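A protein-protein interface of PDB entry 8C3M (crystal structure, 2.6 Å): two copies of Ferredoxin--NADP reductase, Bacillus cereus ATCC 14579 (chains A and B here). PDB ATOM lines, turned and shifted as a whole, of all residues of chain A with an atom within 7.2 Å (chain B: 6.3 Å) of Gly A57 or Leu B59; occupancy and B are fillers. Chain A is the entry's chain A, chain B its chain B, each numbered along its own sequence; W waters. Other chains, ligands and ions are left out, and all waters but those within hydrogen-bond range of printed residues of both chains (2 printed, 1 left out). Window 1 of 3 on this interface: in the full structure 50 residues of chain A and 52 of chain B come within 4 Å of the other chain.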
ATOM      1  N   PHE A  23     -18.973   5.755  15.011  1.00  0.00           N
ATOM      2  CA  PHE A  23     -19.722   6.658  14.137  1.00  0.00           C
ATOM      3  C   PHE A  23     -20.537   5.865  13.120  1.00  0.00           C
ATOM      4  O   PHE A  23     -21.758   6.035  13.018  1.00  0.00           O
ATOM      5  CB  PHE A  23     -18.780   7.655  13.437  1.00  0.00           C
ATOM      6  CG  PHE A  23     -19.375   8.284  12.195  1.00  0.00           C
ATOM      7  CD1 PHE A  23     -20.246   9.345  12.283  1.00  0.00           C
ATOM      8  CD2 PHE A  23     -19.053   7.810  10.941  1.00  0.00           C
ATOM      9  CE1 PHE A  23     -20.805   9.909  11.139  1.00  0.00           C
ATOM     10  CE2 PHE A  23     -19.608   8.374   9.794  1.00  0.00           C
ATOM     11  CZ  PHE A  23     -20.487   9.416   9.905  1.00  0.00           C
ATOM     12  N   TRP A  54      -0.491  14.514   6.851  1.00  0.00           N
ATOM     13  CA  TRP A  54      -0.841  14.884   5.485  1.00  0.00           C
ATOM     14  C   TRP A  54      -1.632  13.838   4.710  1.00  0.00           C
ATOM     15  O   TRP A  54      -2.224  14.192   3.681  1.00  0.00           O
ATOM     16  CB  TRP A  54       0.433  15.169   4.675  1.00  0.00           C
ATOM     17  CG  TRP A  54       1.231  16.317   5.152  1.00  0.00           C
ATOM     18  CD1 TRP A  54       1.971  16.378   6.296  1.00  0.00           C
ATOM     19  CD2 TRP A  54       1.414  17.564   4.482  1.00  0.00           C
ATOM     20  NE1 TRP A  54       2.589  17.591   6.386  1.00  0.00           N
ATOM     21  CE2 TRP A  54       2.278  18.337   5.278  1.00  0.00           C
ATOM     22  CE3 TRP A  54       0.946  18.096   3.278  1.00  0.00           C
ATOM     23  CZ2 TRP A  54       2.667  19.629   4.925  1.00  0.00           C
ATOM     24  CZ3 TRP A  54       1.354  19.381   2.916  1.00  0.00           C
ATOM     25  CH2 TRP A  54       2.193  20.132   3.745  1.00  0.00           C
ATOM     26  N   ASP A  55      -1.624  12.565   5.142  1.00  0.00           N
ATOM     27  CA  ASP A  55      -2.097  11.453   4.324  1.00  0.00           C
ATOM     28  C   ASP A  55      -3.404  10.838   4.821  1.00  0.00           C
ATOM     29  O   ASP A  55      -3.709   9.687   4.491  1.00  0.00           O
ATOM     30  CB  ASP A  55      -1.022  10.373   4.233  1.00  0.00           C
ATOM     31  CG  ASP A  55      -0.512   9.929   5.608  1.00  0.00           C
ATOM     32  OD1 ASP A  55      -1.089  10.346   6.635  1.00  0.00           O
ATOM     33  OD2 ASP A  55       0.477   9.156   5.654  1.00  0.00           O
ATOM     34  N   VAL A  56      -4.206  11.582   5.566  1.00  0.00           N
ATOM     35  CA  VAL A  56      -5.589  11.201   5.807  1.00  0.00           C
ATOM     36  C   VAL A  56      -6.412  11.762   4.660  1.00  0.00           C
ATOM     37  O   VAL A  56      -6.324  12.960   4.343  1.00  0.00           O
ATOM     38  CB  VAL A  56      -6.073  11.730   7.161  1.00  0.00           C
ATOM     39  CG1 VAL A  56      -7.531  11.435   7.345  1.00  0.00           C
ATOM     40  CG2 VAL A  56      -5.206  11.154   8.276  1.00  0.00           C
ATOM     41  N   GLY A  57      -7.180  10.896   4.007  1.00  0.00           N
ATOM     42  CA  GLY A  57      -7.841  11.292   2.779  1.00  0.00           C
ATOM     43  C   GLY A  57      -8.747  12.491   2.967  1.00  0.00           C
ATOM     44  O   GLY A  57      -9.625  12.456   3.820  1.00  0.00           O
ATOM     45  N   GLY A  58      -8.508  13.581   2.252  1.00  0.00           N
ATOM     46  CA  GLY A  58      -9.385  14.719   2.356  1.00  0.00           C
ATOM     47  C   GLY A  58      -9.012  15.734   3.412  1.00  0.00           C
ATOM     48  O   GLY A  58      -9.614  16.821   3.434  1.00  0.00           O
ATOM     49  N   LEU A  59      -8.056  15.418   4.295  1.00  0.00           N
ATOM     50  CA  LEU A  59      -7.581  16.376   5.293  1.00  0.00           C
ATOM     51  C   LEU A  59      -6.381  17.161   4.776  1.00  0.00           C
ATOM     52  O   LEU A  59      -5.339  16.577   4.460  1.00  0.00           O
ATOM     53  CB  LEU A  59      -7.164  15.709   6.595  1.00  0.00           C
ATOM     54  CG  LEU A  59      -8.123  15.709   7.766  1.00  0.00           C
ATOM     55  CD1 LEU A  59      -9.269  14.722   7.548  1.00  0.00           C
ATOM     56  CD2 LEU A  59      -7.333  15.418   9.054  1.00  0.00           C
ATOM     57  N   LEU A  60      -6.513  18.483   4.753  1.00  0.00           N
ATOM     58  CA  LEU A  60      -5.345  19.333   4.651  1.00  0.00           C
ATOM     59  C   LEU A  60      -4.475  19.163   5.898  1.00  0.00           C
ATOM     60  O   LEU A  60      -4.982  18.875   6.983  1.00  0.00           O
ATOM     61  CB  LEU A  60      -5.790  20.778   4.473  1.00  0.00           C
ATOM     62  CG  LEU A  60      -6.569  20.869   3.156  1.00  0.00           C
ATOM     63  CD1 LEU A  60      -7.003  22.266   2.839  1.00  0.00           C
ATOM     64  CD2 LEU A  60      -5.724  20.306   1.994  1.00  0.00           C
ATOM     65  N   LEU A  67      -6.289  16.436  14.810  1.00  0.00           N
ATOM     66  CA  LEU A  67      -6.912  15.224  14.272  1.00  0.00           C
ATOM     67  C   LEU A  67      -7.644  14.434  15.351  1.00  0.00           C
ATOM     68  O   LEU A  67      -8.758  13.948  15.118  1.00  0.00           O
ATOM     69  CB  LEU A  67      -5.862  14.352  13.584  1.00  0.00           C
ATOM     70  CG  LEU A  67      -6.393  13.062  12.968  1.00  0.00           C
ATOM     71  CD1 LEU A  67      -7.561  13.359  12.069  1.00  0.00           C
ATOM     72  CD2 LEU A  67      -5.325  12.325  12.179  1.00  0.00           C
ATOM     73  N   GLN A  70     -10.917  16.168  15.829  1.00  0.00           N
ATOM     74  CA  GLN A  70     -11.896  15.883  14.780  1.00  0.00           C
ATOM     75  C   GLN A  70     -12.441  14.452  14.871  1.00  0.00           C
ATOM     76  O   GLN A  70     -13.658  14.233  14.759  1.00  0.00           O
ATOM     77  CB  GLN A  70     -11.266  16.153  13.412  1.00  0.00           C
ATOM     78  CG  GLN A  70     -11.137  17.653  13.127  1.00  0.00           C
ATOM     79  CD  GLN A  70     -10.264  17.983  11.917  1.00  0.00           C
ATOM     80  OE1 GLN A  70      -9.386  18.849  11.997  1.00  0.00           O
ATOM     81  NE2 GLN A  70     -10.495  17.311  10.800  1.00  0.00           N
ATOM     82  N   LEU A  71     -11.570  13.465  15.098  1.00  0.00           N
ATOM     83  CA  LEU A  71     -12.042  12.079  15.124  1.00  0.00           C
ATOM     84  C   LEU A  71     -12.972  11.824  16.305  1.00  0.00           C
ATOM     85  O   LEU A  71     -14.011  11.163  16.166  1.00  0.00           O
ATOM     86  CB  LEU A  71     -10.851  11.121  15.170  1.00  0.00           C
ATOM     87  CG  LEU A  71     -10.035  11.107  13.885  1.00  0.00           C
ATOM     88  CD1 LEU A  71      -8.677  10.476  14.116  1.00  0.00           C
ATOM     89  CD2 LEU A  71     -10.834  10.378  12.833  1.00  0.00           C
ATOM     90  N   GLN A  74     -16.337  13.162  15.506  1.00  0.00           N
ATOM     91  CA  GLN A  74     -17.079  12.331  14.578  1.00  0.00           C
ATOM     92  C   GLN A  74     -17.533  11.040  15.257  1.00  0.00           C
ATOM     93  O   GLN A  74     -18.700  10.644  15.121  1.00  0.00           O
ATOM     94  CB  GLN A  74     -16.236  12.064  13.334  1.00  0.00           C
ATOM     95  CG  GLN A  74     -16.921  11.258  12.217  1.00  0.00           C
ATOM     96  CD  GLN A  74     -15.962  10.952  11.096  1.00  0.00           C
ATOM     97  OE1 GLN A  74     -14.801  10.638  11.351  1.00  0.00           O
ATOM     98  NE2 GLN A  74     -16.436  11.027   9.847  1.00  0.00           N
ATOM     99  N   ILE A 301      -3.999   5.540   8.848  1.00  0.00           N
ATOM    100  CA  ILE A 301      -5.279   5.948   9.406  1.00  0.00           C
ATOM    101  C   ILE A 301      -6.367   5.788   8.356  1.00  0.00           C
ATOM    102  O   ILE A 301      -7.477   5.324   8.653  1.00  0.00           O
ATOM    103  CB  ILE A 301      -5.207   7.379   9.956  1.00  0.00           C
ATOM    104  CG1 ILE A 301      -4.295   7.409  11.179  1.00  0.00           C
ATOM    105  CG2 ILE A 301      -6.619   7.893  10.301  1.00  0.00           C
ATOM    106  CD1 ILE A 301      -3.728   8.837  11.485  1.00  0.00           C
ATOM    107  N   ALA A 302      -6.048   6.119   7.101  1.00  0.00           N
ATOM    108  CA  ALA A 302      -7.015   5.927   6.029  1.00  0.00           C
ATOM    109  C   ALA A 302      -7.528   4.484   5.985  1.00  0.00           C
ATOM    110  O   ALA A 302      -8.730   4.256   5.824  1.00  0.00           O
ATOM    111  CB  ALA A 302      -6.398   6.338   4.690  1.00  0.00           C
ATOM    112  N   PHE A 305     -10.304   3.530   8.551  1.00  0.00           N
ATOM    113  CA  PHE A 305     -11.686   3.873   8.199  1.00  0.00           C
ATOM    114  C   PHE A 305     -12.324   2.784   7.353  1.00  0.00           C
ATOM    115  O   PHE A 305     -13.499   2.436   7.551  1.00  0.00           O
ATOM    116  CB  PHE A 305     -11.739   5.218   7.464  1.00  0.00           C
ATOM    117  CG  PHE A 305     -11.134   6.335   8.236  1.00  0.00           C
ATOM    118  CD1 PHE A 305     -11.282   6.385   9.623  1.00  0.00           C
ATOM    119  CD2 PHE A 305     -10.375   7.324   7.581  1.00  0.00           C
ATOM    120  CE1 PHE A 305     -10.720   7.425  10.358  1.00  0.00           C
ATOM    121  CE2 PHE A 305      -9.772   8.370   8.296  1.00  0.00           C
ATOM    122  CZ  PHE A 305      -9.956   8.426   9.693  1.00  0.00           C
ATOM    123  N   TYR B  20      -6.319  11.185  -4.601  1.00  0.00           N
ATOM    124  CA  TYR B  20      -5.511  10.594  -3.548  1.00  0.00           C
ATOM    125  C   TYR B  20      -4.435   9.689  -4.135  1.00  0.00           C
ATOM    126  O   TYR B  20      -3.360   9.550  -3.534  1.00  0.00           O
ATOM    127  CB  TYR B  20      -6.400   9.843  -2.562  1.00  0.00           C
ATOM    128  CG  TYR B  20      -5.665   9.475  -1.305  1.00  0.00           C
ATOM    129  CD1 TYR B  20      -5.481  10.390  -0.260  1.00  0.00           C
ATOM    130  CD2 TYR B  20      -5.097   8.217  -1.179  1.00  0.00           C
ATOM    131  CE1 TYR B  20      -4.772  10.024   0.888  1.00  0.00           C
ATOM    132  CE2 TYR B  20      -4.388   7.852  -0.057  1.00  0.00           C
ATOM    133  CZ  TYR B  20      -4.228   8.737   0.968  1.00  0.00           C
ATOM    134  OH  TYR B  20      -3.517   8.283   2.052  1.00  0.00           O
ATOM    135  N   ILE B  53     -21.469  16.376   4.077  1.00  0.00           N
ATOM    136  CA  ILE B  53     -20.861  15.050   4.020  1.00  0.00           C
ATOM    137  C   ILE B  53     -20.244  14.741   5.373  1.00  0.00           C
ATOM    138  O   ILE B  53     -19.291  15.396   5.805  1.00  0.00           O
ATOM    139  CB  ILE B  53     -19.841  14.964   2.882  1.00  0.00           C
ATOM    140  CG1 ILE B  53     -20.594  15.222   1.576  1.00  0.00           C
ATOM    141  CG2 ILE B  53     -19.139  13.625   2.872  1.00  0.00           C
ATOM    142  CD1 ILE B  53     -19.705  15.599   0.467  1.00  0.00           C
ATOM    143  N   TRP B  54     -20.779  13.718   6.021  1.00  0.00           N
ATOM    144  CA  TRP B  54     -20.460  13.367   7.392  1.00  0.00           C
ATOM    145  C   TRP B  54     -19.549  12.162   7.525  1.00  0.00           C
ATOM    146  O   TRP B  54     -18.959  11.980   8.602  1.00  0.00           O
ATOM    147  CB  TRP B  54     -21.745  13.047   8.153  1.00  0.00           C
ATOM    148  CG  TRP B  54     -22.674  14.160   8.290  1.00  0.00           C
ATOM    149  CD1 TRP B  54     -23.475  14.705   7.321  1.00  0.00           C
ATOM    150  CD2 TRP B  54     -22.916  14.893   9.482  1.00  0.00           C
ATOM    151  NE1 TRP B  54     -24.215  15.740   7.857  1.00  0.00           N
ATOM    152  CE2 TRP B  54     -23.883  15.879   9.180  1.00  0.00           C
ATOM    153  CE3 TRP B  54     -22.410  14.814  10.782  1.00  0.00           C
ATOM    154  CZ2 TRP B  54     -24.356  16.769  10.131  1.00  0.00           C
ATOM    155  CZ3 TRP B  54     -22.893  15.711  11.740  1.00  0.00           C
ATOM    156  CH2 TRP B  54     -23.854  16.670  11.406  1.00  0.00           C
ATOM    157  N   ASP B  55     -19.442  11.321   6.483  1.00  0.00           N
ATOM    158  CA  ASP B  55     -18.824  10.003   6.617  1.00  0.00           C
ATOM    159  C   ASP B  55     -17.471   9.863   5.908  1.00  0.00           C
ATOM    160  O   ASP B  55     -17.077   8.761   5.513  1.00  0.00           O
ATOM    161  CB  ASP B  55     -19.786   8.916   6.160  1.00  0.00           C
ATOM    162  CG  ASP B  55     -20.338   9.165   4.775  1.00  0.00           C
ATOM    163  OD1 ASP B  55     -19.844  10.095   4.078  1.00  0.00           O
ATOM    164  OD2 ASP B  55     -21.303   8.416   4.409  1.00  0.00           O
ATOM    165  N   VAL B  56     -16.737  10.956   5.729  1.00  0.00           N
ATOM    166  CA  VAL B  56     -15.323  10.855   5.418  1.00  0.00           C
ATOM    167  C   VAL B  56     -14.575  10.835   6.743  1.00  0.00           C
ATOM    168  O   VAL B  56     -14.821  11.678   7.608  1.00  0.00           O
ATOM    169  CB  VAL B  56     -14.883  12.015   4.524  1.00  0.00           C
ATOM    170  CG1 VAL B  56     -13.394  11.974   4.281  1.00  0.00           C
ATOM    171  CG2 VAL B  56     -15.640  11.960   3.227  1.00  0.00           C
ATOM    172  N   GLY B  57     -13.737   9.823   6.951  1.00  0.00           N
ATOM    173  CA  GLY B  57     -13.055   9.635   8.221  1.00  0.00           C
ATOM    174  C   GLY B  57     -12.163  10.808   8.589  1.00  0.00           C
ATOM    175  O   GLY B  57     -11.223  11.140   7.855  1.00  0.00           O
ATOM    176  N   GLY B  58     -12.434  11.432   9.732  1.00  0.00           N
ATOM    177  CA  GLY B  58     -11.655  12.547  10.188  1.00  0.00           C
ATOM    178  C   GLY B  58     -12.199  13.899   9.804  1.00  0.00           C
ATOM    179  O   GLY B  58     -11.695  14.908  10.309  1.00  0.00           O
ATOM    180  N   LEU B  59     -13.198  13.962   8.922  1.00  0.00           N
ATOM    181  CA  LEU B  59     -13.825  15.231   8.544  1.00  0.00           C
ATOM    182  C   LEU B  59     -15.071  15.482   9.376  1.00  0.00           C
ATOM    183  O   LEU B  59     -16.027  14.692   9.324  1.00  0.00           O
ATOM    184  CB  LEU B  59     -14.231  15.222   7.078  1.00  0.00           C
ATOM    185  CG  LEU B  59     -13.336  15.774   5.984  1.00  0.00           C
ATOM    186  CD1 LEU B  59     -12.104  14.885   5.788  1.00  0.00           C
ATOM    187  CD2 LEU B  59     -14.174  15.793   4.692  1.00  0.00           C
ATOM    188  N   LEU B  60     -15.082  16.603  10.097  1.00  0.00           N
ATOM    189  CA  LEU B  60     -16.346  17.147  10.566  1.00  0.00           C
ATOM    190  C   LEU B  60     -17.184  17.533   9.350  1.00  0.00           C
ATOM    191  O   LEU B  60     -16.639  17.758   8.268  1.00  0.00           O
ATOM    192  CB  LEU B  60     -16.114  18.344  11.472  1.00  0.00           C
ATOM    193  CG  LEU B  60     -15.342  17.898  12.707  1.00  0.00           C
ATOM    194  CD1 LEU B  60     -15.231  19.033  13.709  1.00  0.00           C
ATOM    195  CD2 LEU B  60     -15.998  16.659  13.328  1.00  0.00           C
ATOM    196  N   PRO B  61     -18.507  17.545   9.469  1.00  0.00           N
ATOM    197  CA  PRO B  61     -19.343  17.707   8.272  1.00  0.00           C
ATOM    198  C   PRO B  61     -18.950  18.941   7.474  1.00  0.00           C
ATOM    199  O   PRO B  61     -18.752  20.038   8.019  1.00  0.00           O
ATOM    200  CB  PRO B  61     -20.763  17.818   8.831  1.00  0.00           C
ATOM    201  CG  PRO B  61     -20.612  17.988  10.285  1.00  0.00           C
ATOM    202  CD  PRO B  61     -19.309  17.372  10.683  1.00  0.00           C
ATOM    203  N   VAL B  62     -18.781  18.733   6.171  1.00  0.00           N
ATOM    204  CA  VAL B  62     -18.450  19.784   5.220  1.00  0.00           C
ATOM    205  C   VAL B  62     -19.407  19.631   4.048  1.00  0.00           C
ATOM    206  O   VAL B  62     -20.023  18.582   3.851  1.00  0.00           O
ATOM    207  CB  VAL B  62     -16.973  19.714   4.735  1.00  0.00           C
ATOM    208  CG1 VAL B  62     -16.002  19.976   5.899  1.00  0.00           C
ATOM    209  CG2 VAL B  62     -16.687  18.370   4.100  1.00  0.00           C
ATOM    210  N   LEU B  67     -15.378  19.980   0.394  1.00  0.00           N
ATOM    211  CA  LEU B  67     -14.642  18.724   0.277  1.00  0.00           C
ATOM    212  C   LEU B  67     -13.857  18.656  -1.033  1.00  0.00           C
ATOM    213  O   LEU B  67     -12.690  18.242  -1.050  1.00  0.00           O
ATOM    214  CB  LEU B  67     -15.617  17.550   0.388  1.00  0.00           C
ATOM    215  CG  LEU B  67     -14.960  16.179   0.270  1.00  0.00           C
ATOM    216  CD1 LEU B  67     -13.827  16.075   1.260  1.00  0.00           C
ATOM    217  CD2 LEU B  67     -15.949  15.060   0.477  1.00  0.00           C
ATOM    218  N   GLN B  70     -10.700  20.684  -0.573  1.00  0.00           N
ATOM    219  CA  GLN B  70      -9.678  19.998   0.203  1.00  0.00           C
ATOM    220  C   GLN B  70      -9.020  18.870  -0.600  1.00  0.00           C
ATOM    221  O   GLN B  70      -7.797  18.711  -0.560  1.00  0.00           O
ATOM    222  CB  GLN B  70     -10.297  19.503   1.511  1.00  0.00           C
ATOM    223  CG  GLN B  70     -10.538  20.651   2.489  1.00  0.00           C
ATOM    224  CD  GLN B  70     -11.407  20.256   3.680  1.00  0.00           C
ATOM    225  OE1 GLN B  70     -12.373  20.958   3.996  1.00  0.00           O
ATOM    226  NE2 GLN B  70     -11.069  19.154   4.358  1.00  0.00           N
ATOM    227  N   LEU B  71      -9.811  18.079  -1.339  1.00  0.00           N
ATOM    228  CA  LEU B  71      -9.251  16.948  -2.086  1.00  0.00           C
ATOM    229  C   LEU B  71      -8.369  17.419  -3.226  1.00  0.00           C
ATOM    230  O   LEU B  71      -7.298  16.850  -3.477  1.00  0.00           O
ATOM    231  CB  LEU B  71     -10.360  16.067  -2.642  1.00  0.00           C
ATOM    232  CG  LEU B  71     -11.179  15.319  -1.613  1.00  0.00           C
ATOM    233  CD1 LEU B  71     -12.443  14.788  -2.279  1.00  0.00           C
ATOM    234  CD2 LEU B  71     -10.341  14.245  -1.031  1.00  0.00           C
ATOM    235  N   GLN B  74      -5.136  18.478  -1.781  1.00  0.00           N
ATOM    236  CA  GLN B  74      -4.299  17.361  -1.365  1.00  0.00           C
ATOM    237  C   GLN B  74      -3.696  16.668  -2.586  1.00  0.00           C
ATOM    238  O   GLN B  74      -2.485  16.395  -2.624  1.00  0.00           O
ATOM    239  CB  GLN B  74      -5.115  16.394  -0.493  1.00  0.00           C
ATOM    240  CG  GLN B  74      -4.339  15.244   0.154  1.00  0.00           C
ATOM    241  CD  GLN B  74      -5.237  14.288   0.948  1.00  0.00           C
ATOM    242  OE1 GLN B  74      -6.349  13.916   0.512  1.00  0.00           O
ATOM    243  NE2 GLN B  74      -4.752  13.875   2.125  1.00  0.00           N
ATOM    244  N   PHE B 305     -10.030   6.165  -0.851  1.00  0.00           N
ATOM    245  CA  PHE B 305      -8.695   6.436  -0.330  1.00  0.00           C
ATOM    246  C   PHE B 305      -7.934   5.145  -0.127  1.00  0.00           C
ATOM    247  O   PHE B 305      -6.742   5.056  -0.463  1.00  0.00           O
ATOM    248  CB  PHE B 305      -8.769   7.193   0.994  1.00  0.00           C
ATOM    249  CG  PHE B 305      -9.513   8.467   0.916  1.00  0.00           C
ATOM    250  CD1 PHE B 305      -9.445   9.264  -0.236  1.00  0.00           C
ATOM    251  CD2 PHE B 305     -10.242   8.915   2.003  1.00  0.00           C
ATOM    252  CE1 PHE B 305     -10.129  10.509  -0.307  1.00  0.00           C
ATOM    253  CE2 PHE B 305     -10.938  10.160   1.958  1.00  0.00           C
ATOM    254  CZ  PHE B 305     -10.881  10.950   0.796  1.00  0.00           C
HETATM  255  O   HOH W   1     -18.441  13.760  10.169  1.00  0.00           O
HETATM  256  O   HOH W   2     -10.360  10.606   5.318  1.00  0.00           O
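O of Trp A54 is in hydrogen-bond range of NE2 of Gln B74, 3.0 Å away. OH of Tyr B20 lies within hydrogen-bond range of O of Asp A55, 2.8 Å away. The side-chain amide nitrogen (NE2) of Gln B74 lies within hydrogen-bond range of the backbone carbonyl oxygen (O) of Val A56. The backbone carbonyl oxygen (O) of Gly A58 sits at hydrogen-bond distance from the side-chain amide nitrogen (NE2) of Gln B70, 2.9 Å away. The backbone NH (N) of Gly A58 lies within hydrogen-bond range of the side-chain amide oxygen (OE1) of Gln B74 (2.8 Å). NE2 of Gln A70 sits at hydrogen-bond distance from O of Gly B58. O of Trp B54 sits at hydrogen-bond distance from NE2 of Gln A74 (3.0 Å). The side-chain amide nitrogen of Gln A74 sits at hydrogen-bond distance from the backbone carbonyl oxygen of Val B56 (2.8 Å). OE1 of Gln A74 sits at hydrogen-bond distance from N of Gly B58 (3.0 Å).
Among the printed residues, merely in contact across the chains: Phe A23 with Trp B54 (3.3 Å), Phe A23 with Asp B55 (3.7 Å), Val A56 with Gly B57 (3.7 Å), Gly A57 with Tyr B20 (3.8 Å), Gly A57 with Val B56 (3.8 Å), Gly A57 with Leu B59 (3.99 Å), Gly A57 with Gln B74 (3.7 Å), Gly A57 with Phe B305 (3.2 Å), Gly A58 with Leu B59 (3.9 Å), Gly A58 with Leu B71 (3.6 Å), Gly A58 with Phe B305 (3.8 Å), Leu A59 with Gly B58 (3.7 Å), Leu A59 with Leu B59 (3.3 Å), Leu A59 with Gln B74 (3.6 Å), Leu A60 with Gln B70 (3.7 Å), Gln A70 with Leu B60 (3.7 Å), Leu A71 with Gly B58 (3.5 Å), Gln A74 with Gly B57 (3.7 Å), Gln A74 with Leu B59 (3.7 Å), Phe A305 with Gly B57 (3.2 Å) and Phe A305 with Gly B58 (3.9 Å).
Water W1 lies within hydrogen-bond range of O of Trp B54 (2.4 Å), O of Leu B59 (2.7 Å) and NE2 of Gln A74 (3.4 Å). Water W2 lies within hydrogen-bond range of O of Gly A57 (2.5 Å) and O of Gly B57 (2.7 Å).
Gly A57 touches Leu B59, but with the chains exchanged Leu A59 does not touch Gly B57 (4.1 Å). Gly A57 touches Gln B74, and with the chains exchanged Gln A74 touches Gly B57. Gly A58 touches Gln B70, and with the chains exchanged Gln A70 touches Gly B58. Leu A59 touches its own counterpart, Leu B59. 12 positions are printed for both chains. Of the 30 pairs that touch across the chains among the printed residues, 25 have their exchanged pair printed and touching as well.
Printed residues of chain B within 4 Å of Gly A57: Tyr B20 (3.8 Å), Val B56 (3.8 Å), Leu B59 (3.99 Å), Gln B74 (3.7 Å) and Phe B305 (3.2 Å). Of the printed residues of chain B, Gln A74 touches Trp B54 (3.0 Å), Val B56 (2.8 Å), Gly B57 (3.7 Å), Gly B58 (3.0 Å) and Leu B59 (3.7 Å). Printed residues of chain A within 4 Å of Leu B59: Gly A57 (3.99 Å), Gly A58 (3.9 Å), Leu A59 (3.3 Å) and Gln A74 (3.7 Å). Of the printed residues of chain A, Leu B60 touches Gln A70 (3.7 Å). Val B62 touches none of the printed residues of chain A. Of the printed residues of chain A, Gln B74 touches Trp A54 (3.0 Å), Val A56 (2.9 Å), Gly A57 (3.7 Å), Gly A58 (2.8 Å) and Leu A59 (3.6 Å). The nearest printed residue of chain B that does not touch Val A56 is Tyr B20 (4.5 Å).
Printed residues of chain B that touch a printed residue of chain A: Tyr B20, Trp B54, Asp B55, Val B56, Gly B57, Gly B58, Leu B59, Leu B60, Gln B70, Leu B71, Gln B74 and Phe B305. Hydrophobic or aromatic side chains of chain B within 4 Å of the printed part of chain A: Tyr B20, Val B56, Leu B59, Leu B60, Leu B71 and Phe B305. Hydrophobic or aromatic side chains of chain A within 4 Å of the printed part of chain B: Phe A23, Val A56, Leu A59, Leu A60, Leu A71 and Phe A305. Along chain A the printed residues that touch a printed residue of chain B span positions 23 to 305. Among the printed residues, 30 pairs touch across the chains. Among the printed residues, no Asp or Glu carboxylate lies within 4 Å of a Lys or Arg side-chain nitrogen of the other chain.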
